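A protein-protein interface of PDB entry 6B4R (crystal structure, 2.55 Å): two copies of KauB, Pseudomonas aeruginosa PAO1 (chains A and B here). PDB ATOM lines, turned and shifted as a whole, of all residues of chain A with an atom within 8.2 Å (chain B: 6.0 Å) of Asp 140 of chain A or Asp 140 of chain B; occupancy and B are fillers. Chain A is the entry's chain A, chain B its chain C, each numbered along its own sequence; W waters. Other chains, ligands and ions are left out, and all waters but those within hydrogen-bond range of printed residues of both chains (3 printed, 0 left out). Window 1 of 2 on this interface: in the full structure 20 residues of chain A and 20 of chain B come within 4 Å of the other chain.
O of Val 142 of chain B lies within hydrogen-bond range of N of Asp 140 of chain A.
The backbone carbonyl oxygen of Val 142 of chain A lies within hydrogen-bond range of the backbone NH of Asp 140 of chain B (2.7 Å).
The backbone carbonyl oxygen (O) of Glu 141 of chain B sits at hydrogen-bond distance from the backbone NH (N) of Val 153 of chain B.
The side-chain carboxylate (OD2) of Asp 140 of chain B is in hydrogen-bond range of the backbone NH (N) of Arg 155 of chain B, 3.2 Å away.
The backbone NH (N) of Ala 143 of chain A lies within hydrogen-bond range of the backbone carbonyl oxygen (O) of Gly 151 of chain A, 2.9 Å away.
OD2 of Asp 140 of chain A sits at hydrogen-bond distance from N of Arg 155 of chain A (3.1 Å).
The backbone carbonyl oxygen (O) of Glu 141 of chain A is in hydrogen-bond range of the backbone NH (N) of Val 153 of chain A (2.9 Å).
Among the printed residues, merely in contact across the chains: Tyr 139 of chain A with Glu 141 of chain B, Tyr 139 of chain A with Val 142 of chain B, Tyr 139 of chain A with Ala 143 of chain B, Asp 140 of chain A with Asp 140 of chain B, Asp 140 of chain A with Glu 141 of chain B, Glu 141 of chain A with Tyr 139 of chain B, Glu 141 of chain A with Asp 140 of chain B, Glu 141 of chain A with Val 142 of chain B, Val 142 of chain A with Tyr 139 of chain B, Val 142 of chain A with Glu 141 of chain B, Val 142 of chain A with Val 142 of chain B and Ala 143 of chain A with Tyr 139 of chain B.
Of the printed residues of chain B, Tyr 139 of chain A touches Glu 141, Val 142 and Ala 143.
Asp 140 of chain A touches just these residues of chain B: Asp 140, Glu 141 and Val 142.
Printed residues of chain B within 4 Å of Val 142 of chain A: Tyr 139 (3.3 Å), Asp 140 (2.7 Å), Glu 141 (3.5 Å) and Val 142 (3.6 Å).
Leu 152 of chain A touches none of the printed residues of chain B.
Thr 488 of chain A touches none of the printed residues of chain B.
Printed residues of chain A within 4 Å of Tyr 139 of chain B: Glu 141 (3.95 Å), Val 142 (3.3 Å) and Ala 143 (3.6 Å).
Asp 140 of chain B touches just these residues of chain A: Asp 140, Glu 141 and Val 142.
Printed residues of chain A within 4 Å of Glu 141 of chain B: Tyr 139, Asp 140 and Val 142.
The nearest residue of chain B that does not touch Asp 140 of chain A is Ala 143 of chain B (5.0 Å).
Hydrophobic or aromatic side chains of chain B within 4 Å of the printed part of chain A: Tyr 139, Val 142 and Ala 143.
Of the 21 printed residues of chain A, 5 touch a printed residue of chain B.
Among the printed residues, no Asp or Glu carboxylate lies within 4 Å of a Lys or Arg side-chain nitrogen of the other chain.
Tyr 139 of chain A touches Glu 141 of chain B, and with the chains exchanged Glu 141 of chain A touches Tyr 139 of chain B.
Tyr 139 of chain A touches Val 142 of chain B, and with the chains exchanged Val 142 of chain A touches Tyr 139 of chain B.
Tyr 139 of chain A touches Ala 143 of chain B, and with the chains exchanged Ala 143 of chain A touches Tyr 139 of chain B.
Val 142 of chain A touches its own counterpart, Val 142 of chain B.
Positions printed for both chains: 138, 139, 140, 141, 142, 143, 144, 153, 154 and 155.
Water W1 lies within hydrogen-bond range of N of Ala 144 of chain B (2.7 Å) and O of Ile 138 of chain A (3.2 Å).
Water W3 bridges N of Ala 144 of chain A (3.0 Å) and O of Ile 138 of chain B (3.1 Å).
Water W2 lies within hydrogen-bond range of the backbone carbonyl oxygen (O) of Ile 138 of chain A (3.2 Å), the backbone carbonyl oxygen (O) of Val 142 of chain B (3.4 Å) and the backbone NH (N) of Ala 144 of chain B (3.4 Å).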
ATOM      1  N   LYS A 137     -33.719  -5.291 -18.581  1.00  0.00           N
ATOM      2  CA  LYS A 137     -33.559  -6.343 -19.581  1.00  0.00           C
ATOM      3  C   LYS A 137     -32.233  -7.057 -19.362  1.00  0.00           C
ATOM      4  O   LYS A 137     -31.975  -8.106 -19.950  1.00  0.00           O
ATOM      5  CB  LYS A 137     -33.622  -5.773 -21.001  1.00  0.00           C
ATOM      6  CG  LYS A 137     -34.824  -4.879 -21.268  1.00  0.00           C
ATOM      7  CD  LYS A 137     -36.132  -5.589 -20.942  1.00  0.00           C
ATOM      8  CE  LYS A 137     -37.336  -4.722 -21.284  1.00  0.00           C
ATOM      9  NZ  LYS A 137     -37.293  -3.405 -20.586  1.00  0.00           N
ATOM     10  N   ILE A 138     -31.397  -6.472 -18.509  1.00  0.00           N
ATOM     11  CA  ILE A 138     -30.087  -7.033 -18.201  1.00  0.00           C
ATOM     12  C   ILE A 138     -30.180  -8.015 -17.041  1.00  0.00           C
ATOM     13  O   ILE A 138     -30.794  -7.722 -16.015  1.00  0.00           O
ATOM     14  CB  ILE A 138     -29.072  -5.929 -17.845  1.00  0.00           C
ATOM     15  CG1 ILE A 138     -28.941  -4.936 -19.001  1.00  0.00           C
ATOM     16  CG2 ILE A 138     -27.715  -6.532 -17.508  1.00  0.00           C
ATOM     17  CD1 ILE A 138     -28.050  -3.754 -18.690  1.00  0.00           C
ATOM     18  N   TYR A 139     -29.565  -9.179 -17.209  1.00  0.00           N
ATOM     19  CA  TYR A 139     -29.591 -10.214 -16.185  1.00  0.00           C
ATOM     20  C   TYR A 139     -28.196 -10.500 -15.646  1.00  0.00           C
ATOM     21  O   TYR A 139     -27.247 -10.651 -16.415  1.00  0.00           O
ATOM     22  CB  TYR A 139     -30.194 -11.501 -16.752  1.00  0.00           C
ATOM     23  CG  TYR A 139     -31.692 -11.447 -16.961  1.00  0.00           C
ATOM     24  CD1 TYR A 139     -32.560 -12.020 -16.042  1.00  0.00           C
ATOM     25  CD2 TYR A 139     -32.238 -10.824 -18.076  1.00  0.00           C
ATOM     26  CE1 TYR A 139     -33.928 -11.976 -16.226  1.00  0.00           C
ATOM     27  CE2 TYR A 139     -33.608 -10.776 -18.268  1.00  0.00           C
ATOM     28  CZ  TYR A 139     -34.446 -11.352 -17.337  1.00  0.00           C
ATOM     29  OH  TYR A 139     -35.809 -11.312 -17.519  1.00  0.00           O
ATOM     30  N   ASP A 140     -28.073 -10.571 -14.324  1.00  0.00           N
ATOM     31  CA  ASP A 140     -26.829 -11.010 -13.700  1.00  0.00           C
ATOM     32  C   ASP A 140     -26.728 -12.533 -13.754  1.00  0.00           C
ATOM     33  O   ASP A 140     -27.561 -13.191 -14.373  1.00  0.00           O
ATOM     34  CB  ASP A 140     -26.714 -10.491 -12.265  1.00  0.00           C
ATOM     35  CG  ASP A 140     -26.468  -8.993 -12.207  1.00  0.00           C
ATOM     36  OD1 ASP A 140     -25.940  -8.440 -13.196  1.00  0.00           O
ATOM     37  OD2 ASP A 140     -26.800  -8.366 -11.177  1.00  0.00           O
ATOM     38  N   GLU A 141     -25.714 -13.097 -13.106  1.00  0.00           N
ATOM     39  CA  GLU A 141     -25.386 -14.502 -13.326  1.00  0.00           C
ATOM     40  C   GLU A 141     -25.536 -15.400 -12.098  1.00  0.00           C
ATOM     41  O   GLU A 141     -25.432 -14.944 -10.959  1.00  0.00           O
ATOM     42  CB  GLU A 141     -23.963 -14.620 -13.884  1.00  0.00           C
ATOM     43  CG  GLU A 141     -23.724 -13.786 -15.137  1.00  0.00           C
ATOM     44  CD  GLU A 141     -22.250 -13.665 -15.494  1.00  0.00           C
ATOM     45  OE1 GLU A 141     -21.400 -13.750 -14.581  1.00  0.00           O
ATOM     46  OE2 GLU A 141     -21.941 -13.486 -16.689  1.00  0.00           O
ATOM     47  N   VAL A 142     -25.793 -16.680 -12.357  1.00  0.00           N
ATOM     48  CA  VAL A 142     -25.724 -17.725 -11.341  1.00  0.00           C
ATOM     49  C   VAL A 142     -24.763 -18.798 -11.834  1.00  0.00           C
ATOM     50  O   VAL A 142     -24.965 -19.372 -12.905  1.00  0.00           O
ATOM     51  CB  VAL A 142     -27.093 -18.378 -11.082  1.00  0.00           C
ATOM     52  CG1 VAL A 142     -26.956 -19.487 -10.050  1.00  0.00           C
ATOM     53  CG2 VAL A 142     -28.104 -17.343 -10.623  1.00  0.00           C
ATOM     54  N   ALA A 143     -23.719 -19.071 -11.060  1.00  0.00           N
ATOM     55  CA  ALA A 143     -22.685 -20.000 -11.504  1.00  0.00           C
ATOM     56  C   ALA A 143     -23.069 -21.460 -11.300  1.00  0.00           C
ATOM     57  O   ALA A 143     -23.909 -21.788 -10.460  1.00  0.00           O
ATOM     58  CB  ALA A 143     -21.361 -19.702 -10.813  1.00  0.00           C
ATOM     59  N   ALA A 144     -22.444 -22.330 -12.086  1.00  0.00           N
ATOM     60  CA  ALA A 144     -22.603 -23.767 -11.926  1.00  0.00           C
ATOM     61  C   ALA A 144     -21.753 -24.227 -10.748  1.00  0.00           C
ATOM     62  O   ALA A 144     -20.540 -24.387 -10.870  1.00  0.00           O
ATOM     63  CB  ALA A 144     -22.198 -24.493 -13.197  1.00  0.00           C
ATOM     64  N   THR A 145     -22.402 -24.430  -9.608  1.00  0.00           N
ATOM     65  CA  THR A 145     -21.713 -24.793  -8.379  1.00  0.00           C
ATOM     66  C   THR A 145     -22.213 -26.153  -7.896  1.00  0.00           C
ATOM     67  O   THR A 145     -23.193 -26.675  -8.433  1.00  0.00           O
ATOM     68  CB  THR A 145     -21.954 -23.727  -7.284  1.00  0.00           C
ATOM     69  OG1 THR A 145     -23.356 -23.631  -7.000  1.00  0.00           O
ATOM     70  CG2 THR A 145     -21.438 -22.369  -7.737  1.00  0.00           C
ATOM     71  N   LEU A 150     -24.657 -21.937  -3.479  1.00  0.00           N
ATOM     72  CA  LEU A 150     -25.246 -20.990  -4.422  1.00  0.00           C
ATOM     73  C   LEU A 150     -24.264 -19.867  -4.739  1.00  0.00           C
ATOM     74  O   LEU A 150     -23.802 -19.162  -3.842  1.00  0.00           O
ATOM     75  CB  LEU A 150     -26.551 -20.414  -3.868  1.00  0.00           C
ATOM     76  CG  LEU A 150     -27.254 -19.336  -4.700  1.00  0.00           C
ATOM     77  CD1 LEU A 150     -27.705 -19.882  -6.049  1.00  0.00           C
ATOM     78  CD2 LEU A 150     -28.433 -18.750  -3.937  1.00  0.00           C
ATOM     79  N   GLY A 151     -23.952 -19.707  -6.021  1.00  0.00           N
ATOM     80  CA  GLY A 151     -22.990 -18.709  -6.452  1.00  0.00           C
ATOM     81  C   GLY A 151     -23.606 -17.631  -7.321  1.00  0.00           C
ATOM     82  O   GLY A 151     -23.949 -17.868  -8.478  1.00  0.00           O
ATOM     83  N   LEU A 152     -23.740 -16.437  -6.757  1.00  0.00           N
ATOM     84  CA  LEU A 152     -24.330 -15.314  -7.467  1.00  0.00           C
ATOM     85  C   LEU A 152     -23.256 -14.343  -7.934  1.00  0.00           C
ATOM     86  O   LEU A 152     -22.359 -13.979  -7.173  1.00  0.00           O
ATOM     87  CB  LEU A 152     -25.317 -14.577  -6.561  1.00  0.00           C
ATOM     88  CG  LEU A 152     -26.428 -15.423  -5.939  1.00  0.00           C
ATOM     89  CD1 LEU A 152     -27.304 -14.569  -5.037  1.00  0.00           C
ATOM     90  CD2 LEU A 152     -27.258 -16.091  -7.026  1.00  0.00           C
ATOM     91  N   VAL A 153     -23.351 -13.923  -9.190  1.00  0.00           N
ATOM     92  CA  VAL A 153     -22.451 -12.910  -9.717  1.00  0.00           C
ATOM     93  C   VAL A 153     -23.273 -11.709 -10.158  1.00  0.00           C
ATOM     94  O   VAL A 153     -23.871 -11.717 -11.232  1.00  0.00           O
ATOM     95  CB  VAL A 153     -21.619 -13.441 -10.898  1.00  0.00           C
ATOM     96  CG1 VAL A 153     -20.638 -12.380 -11.372  1.00  0.00           C
ATOM     97  CG2 VAL A 153     -20.882 -14.710 -10.495  1.00  0.00           C
ATOM     98  N   THR A 154     -23.304 -10.681  -9.317  1.00  0.00           N
ATOM     99  CA  THR A 154     -24.169  -9.529  -9.543  1.00  0.00           C
ATOM    100  C   THR A 154     -23.384  -8.239  -9.761  1.00  0.00           C
ATOM    101  O   THR A 154     -22.198  -8.159  -9.438  1.00  0.00           O
ATOM    102  CB  THR A 154     -25.152  -9.330  -8.369  1.00  0.00           C
ATOM    103  OG1 THR A 154     -24.420  -9.244  -7.139  1.00  0.00           O
ATOM    104  CG2 THR A 154     -26.132 -10.491  -8.290  1.00  0.00           C
ATOM    105  N   ARG A 155     -24.057  -7.234 -10.314  1.00  0.00           N
ATOM    106  CA  ARG A 155     -23.453  -5.923 -10.526  1.00  0.00           C
ATOM    107  C   ARG A 155     -24.070  -4.866  -9.615  1.00  0.00           C
ATOM    108  O   ARG A 155     -25.270  -4.885  -9.348  1.00  0.00           O
ATOM    109  CB  ARG A 155     -23.579  -5.496 -11.989  1.00  0.00           C
ATOM    110  CG  ARG A 155     -22.720  -6.311 -12.936  1.00  0.00           C
ATOM    111  CD  ARG A 155     -22.590  -5.629 -14.287  1.00  0.00           C
ATOM    112  NE  ARG A 155     -21.614  -6.297 -15.141  1.00  0.00           N
ATOM    113  CZ  ARG A 155     -20.323  -5.985 -15.192  1.00  0.00           C
ATOM    114  NH1 ARG A 155     -19.842  -5.006 -14.434  1.00  0.00           N
ATOM    115  NH2 ARG A 155     -19.511  -6.650 -16.002  1.00  0.00           N
ATOM    116  N   GLU A 156     -23.236  -3.950  -9.134  1.00  0.00           N
ATOM    117  CA  GLU A 156     -23.688  -2.885  -8.247  1.00  0.00           C
ATOM    118  C   GLU A 156     -23.071  -1.565  -8.671  1.00  0.00           C
ATOM    119  O   GLU A 156     -21.922  -1.533  -9.106  1.00  0.00           O
ATOM    120  CB  GLU A 156     -23.295  -3.190  -6.801  1.00  0.00           C
ATOM    121  CG  GLU A 156     -23.948  -4.428  -6.223  1.00  0.00           C
ATOM    122  CD  GLU A 156     -23.439  -4.748  -4.836  1.00  0.00           C
ATOM    123  OE1 GLU A 156     -23.932  -5.721  -4.228  1.00  0.00           O
ATOM    124  OE2 GLU A 156     -22.544  -4.023  -4.355  1.00  0.00           O
ATOM    125  N   ASP A 485     -21.105  -1.415 -17.849  1.00  0.00           N
ATOM    126  CA  ASP A 485     -20.030  -2.055 -17.097  1.00  0.00           C
ATOM    127  C   ASP A 485     -19.037  -1.049 -16.520  1.00  0.00           C
ATOM    128  O   ASP A 485     -18.317  -1.353 -15.569  1.00  0.00           O
ATOM    129  CB  ASP A 485     -19.290  -3.071 -17.971  1.00  0.00           C
ATOM    130  CG  ASP A 485     -20.188  -4.200 -18.446  1.00  0.00           C
ATOM    131  OD1 ASP A 485     -21.248  -4.431 -17.822  1.00  0.00           O
ATOM    132  OD2 ASP A 485     -19.826  -4.862 -19.443  1.00  0.00           O
ATOM    133  N   THR A 488     -20.438  -0.040 -12.923  1.00  0.00           N
ATOM    134  CA  THR A 488     -20.797  -1.078 -11.967  1.00  0.00           C
ATOM    135  C   THR A 488     -19.593  -1.911 -11.544  1.00  0.00           C
ATOM    136  O   THR A 488     -18.583  -1.974 -12.248  1.00  0.00           O
ATOM    137  CB  THR A 488     -21.890  -2.025 -12.511  1.00  0.00           C
ATOM    138  OG1 THR A 488     -21.513  -2.512 -13.806  1.00  0.00           O
ATOM    139  CG2 THR A 488     -23.232  -1.309 -12.602  1.00  0.00           C
ATOM    140  N   GLU A 489     -19.717  -2.540 -10.381  1.00  0.00           N
ATOM    141  CA  GLU A 489     -18.714  -3.469  -9.882  1.00  0.00           C
ATOM    142  C   GLU A 489     -19.301  -4.874  -9.844  1.00  0.00           C
ATOM    143  O   GLU A 489     -20.497  -5.048  -9.622  1.00  0.00           O
ATOM    144  CB  GLU A 489     -18.267  -3.068  -8.475  1.00  0.00           C
ATOM    145  CG  GLU A 489     -17.608  -1.705  -8.379  1.00  0.00           C
ATOM    146  CD  GLU A 489     -16.097  -1.774  -8.488  1.00  0.00           C
ATOM    147  OE1 GLU A 489     -15.415  -1.125  -7.667  1.00  0.00           O
ATOM    148  OE2 GLU A 489     -15.592  -2.476  -9.392  1.00  0.00           O
ATOM    149  N   LEU A 490     -18.455  -5.873 -10.064  1.00  0.00           N
ATOM    150  CA  LEU A 490     -18.875  -7.265  -9.970  1.00  0.00           C
ATOM    151  C   LEU A 490     -18.749  -7.773  -8.540  1.00  0.00           C
ATOM    152  O   LEU A 490     -17.755  -7.516  -7.862  1.00  0.00           O
ATOM    153  CB  LEU A 490     -18.033  -8.135 -10.900  1.00  0.00           C
ATOM    154  CG  LEU A 490     -18.380  -8.050 -12.382  1.00  0.00           C
ATOM    155  CD1 LEU A 490     -17.378  -8.839 -13.204  1.00  0.00           C
ATOM    156  CD2 LEU A 490     -19.788  -8.567 -12.613  1.00  0.00           C
ATOM    157  N   LYS A 491     -19.766  -8.495  -8.085  1.00  0.00           N
ATOM    158  CA  LYS A 491     -19.737  -9.092  -6.758  1.00  0.00           C
ATOM    159  C   LYS A 491     -20.050 -10.579  -6.838  1.00  0.00           C
ATOM    160  O   LYS A 491     -21.115 -10.970  -7.309  1.00  0.00           O
ATOM    161  CB  LYS A 491     -20.734  -8.396  -5.829  1.00  0.00           C
ATOM    162  CG  LYS A 491     -20.954  -9.126  -4.514  1.00  0.00           C
ATOM    163  CD  LYS A 491     -21.893  -8.362  -3.597  1.00  0.00           C
ATOM    164  CE  LYS A 491     -21.265  -7.060  -3.145  1.00  0.00           C
ATOM    165  NZ  LYS A 491     -22.162  -6.305  -2.228  1.00  0.00           N
ATOM    166  N   ILE B 138     -21.444 -22.504 -18.248  1.00  0.00           N
ATOM    167  CA  ILE B 138     -22.774 -21.948 -18.457  1.00  0.00           C
ATOM    168  C   ILE B 138     -23.271 -21.282 -17.180  1.00  0.00           C
ATOM    169  O   ILE B 138     -23.167 -21.850 -16.095  1.00  0.00           O
ATOM    170  CB  ILE B 138     -23.776 -23.042 -18.892  1.00  0.00           C
ATOM    171  CG1 ILE B 138     -23.374 -23.624 -20.249  1.00  0.00           C
ATOM    172  CG2 ILE B 138     -25.192 -22.493 -18.954  1.00  0.00           C
ATOM    173  CD1 ILE B 138     -24.264 -24.752 -20.713  1.00  0.00           C
ATOM    174  N   TYR B 139     -23.802 -20.073 -17.314  1.00  0.00           N
ATOM    175  CA  TYR B 139     -24.305 -19.327 -16.169  1.00  0.00           C
ATOM    176  C   TYR B 139     -25.806 -19.109 -16.285  1.00  0.00           C
ATOM    177  O   TYR B 139     -26.315 -18.823 -17.367  1.00  0.00           O
ATOM    178  CB  TYR B 139     -23.589 -17.979 -16.056  1.00  0.00           C
ATOM    179  CG  TYR B 139     -22.145 -18.091 -15.625  1.00  0.00           C
ATOM    180  CD1 TYR B 139     -21.781 -17.887 -14.299  1.00  0.00           C
ATOM    181  CD2 TYR B 139     -21.148 -18.410 -16.539  1.00  0.00           C
ATOM    182  CE1 TYR B 139     -20.466 -17.993 -13.894  1.00  0.00           C
ATOM    183  CE2 TYR B 139     -19.828 -18.521 -16.144  1.00  0.00           C
ATOM    184  CZ  TYR B 139     -19.492 -18.311 -14.819  1.00  0.00           C
ATOM    185  OH  TYR B 139     -18.178 -18.418 -14.420  1.00  0.00           O
ATOM    186  N   ASP B 140     -26.516 -19.255 -15.170  1.00  0.00           N
ATOM    187  CA  ASP B 140     -27.938 -18.941 -15.132  1.00  0.00           C
ATOM    188  C   ASP B 140     -28.131 -17.447 -14.884  1.00  0.00           C
ATOM    189  O   ASP B 140     -27.186 -16.666 -15.015  1.00  0.00           O
ATOM    190  CB  ASP B 140     -28.661 -19.780 -14.074  1.00  0.00           C
ATOM    191  CG  ASP B 140     -28.794 -21.242 -14.475  1.00  0.00           C
ATOM    192  OD1 ASP B 140     -28.838 -21.530 -15.691  1.00  0.00           O
ATOM    193  OD2 ASP B 140     -28.854 -22.106 -13.575  1.00  0.00           O
ATOM    194  N   GLU B 141     -29.344 -17.048 -14.517  1.00  0.00           N
ATOM    195  CA  GLU B 141     -29.695 -15.632 -14.513  1.00  0.00           C
ATOM    196  C   GLU B 141     -30.169 -15.089 -13.169  1.00  0.00           C
ATOM    197  O   GLU B 141     -30.764 -15.806 -12.363  1.00  0.00           O
ATOM    198  CB  GLU B 141     -30.757 -15.354 -15.584  1.00  0.00           C
ATOM    199  CG  GLU B 141     -30.278 -15.569 -17.012  1.00  0.00           C
ATOM    200  CD  GLU B 141     -31.422 -15.638 -18.010  1.00  0.00           C
ATOM    201  OE1 GLU B 141     -32.452 -16.276 -17.697  1.00  0.00           O
ATOM    202  OE2 GLU B 141     -31.293 -15.059 -19.108  1.00  0.00           O
ATOM    203  N   VAL B 142     -29.888 -13.807 -12.946  1.00  0.00           N
ATOM    204  CA  VAL B 142     -30.455 -13.053 -11.835  1.00  0.00           C
ATOM    205  C   VAL B 142     -31.135 -11.804 -12.390  1.00  0.00           C
ATOM    206  O   VAL B 142     -30.480 -10.935 -12.967  1.00  0.00           O
ATOM    207  CB  VAL B 142     -29.381 -12.622 -10.820  1.00  0.00           C
ATOM    208  CG1 VAL B 142     -30.016 -11.831  -9.682  1.00  0.00           C
ATOM    209  CG2 VAL B 142     -28.638 -13.830 -10.282  1.00  0.00           C
ATOM    210  N   ALA B 143     -32.449 -11.720 -12.216  1.00  0.00           N
ATOM    211  CA  ALA B 143     -33.232 -10.629 -12.787  1.00  0.00           C
ATOM    212  C   ALA B 143     -33.028  -9.305 -12.057  1.00  0.00           C
ATOM    213  O   ALA B 143     -32.680  -9.279 -10.875  1.00  0.00           O
ATOM    214  CB  ALA B 143     -34.705 -10.994 -12.808  1.00  0.00           C
ATOM    215  N   ALA B 144     -33.245  -8.207 -12.775  1.00  0.00           N
ATOM    216  CA  ALA B 144     -33.233  -6.880 -12.174  1.00  0.00           C
ATOM    217  C   ALA B 144     -34.511  -6.687 -11.368  1.00  0.00           C
ATOM    218  O   ALA B 144     -35.592  -6.522 -11.932  1.00  0.00           O
ATOM    219  CB  ALA B 144     -33.111  -5.811 -13.245  1.00  0.00           C
ATOM    220  N   VAL B 153     -33.235 -17.087 -11.780  1.00  0.00           N
ATOM    221  CA  VAL B 153     -33.723 -17.854 -12.922  1.00  0.00           C
ATOM    222  C   VAL B 153     -32.707 -18.940 -13.267  1.00  0.00           C
ATOM    223  O   VAL B 153     -31.658 -18.658 -13.846  1.00  0.00           O
ATOM    224  CB  VAL B 153     -33.973 -16.954 -14.154  1.00  0.00           C
ATOM    225  CG1 VAL B 153     -34.432 -17.788 -15.346  1.00  0.00           C
ATOM    226  CG2 VAL B 153     -34.996 -15.876 -13.830  1.00  0.00           C
ATOM    227  N   THR B 154     -33.018 -20.180 -12.902  1.00  0.00           N
ATOM    228  CA  THR B 154     -32.062 -21.277 -13.032  1.00  0.00           C
ATOM    229  C   THR B 154     -32.591 -22.432 -13.874  1.00  0.00           C
ATOM    230  O   THR B 154     -33.769 -22.468 -14.228  1.00  0.00           O
ATOM    231  CB  THR B 154     -31.643 -21.829 -11.655  1.00  0.00           C
ATOM    232  OG1 THR B 154     -32.791 -22.360 -10.979  1.00  0.00           O
ATOM    233  CG2 THR B 154     -31.017 -20.730 -10.806  1.00  0.00           C
ATOM    234  N   ARG B 155     -31.707 -23.375 -14.182  1.00  0.00           N
ATOM    235  CA  ARG B 155     -32.065 -24.545 -14.975  1.00  0.00           C
ATOM    236  C   ARG B 155     -31.772 -25.846 -14.234  1.00  0.00           C
ATOM    237  O   ARG B 155     -30.747 -25.980 -13.565  1.00  0.00           O
ATOM    238  CB  ARG B 155     -31.345 -24.522 -16.326  1.00  0.00           C
ATOM    239  CG  ARG B 155     -31.837 -23.422 -17.256  1.00  0.00           C
ATOM    240  CD  ARG B 155     -31.144 -23.470 -18.609  1.00  0.00           C
ATOM    241  NE  ARG B 155     -31.795 -22.604 -19.592  1.00  0.00           N
ATOM    242  CZ  ARG B 155     -32.772 -22.996 -20.404  1.00  0.00           C
ATOM    243  NH1 ARG B 155     -33.216 -24.245 -20.355  1.00  0.00           N
ATOM    244  NH2 ARG B 155     -33.304 -22.141 -21.267  1.00  0.00           N
HETATM  245  O   HOH W   1     -33.886  -8.364 -15.418  1.00  0.00           O
HETATM  246  O   HOH W   2     -29.920  -7.604 -12.963  1.00  0.00           O
HETATM  247  O   HOH W   3     -20.622 -21.402 -14.305  1.00  0.00           O
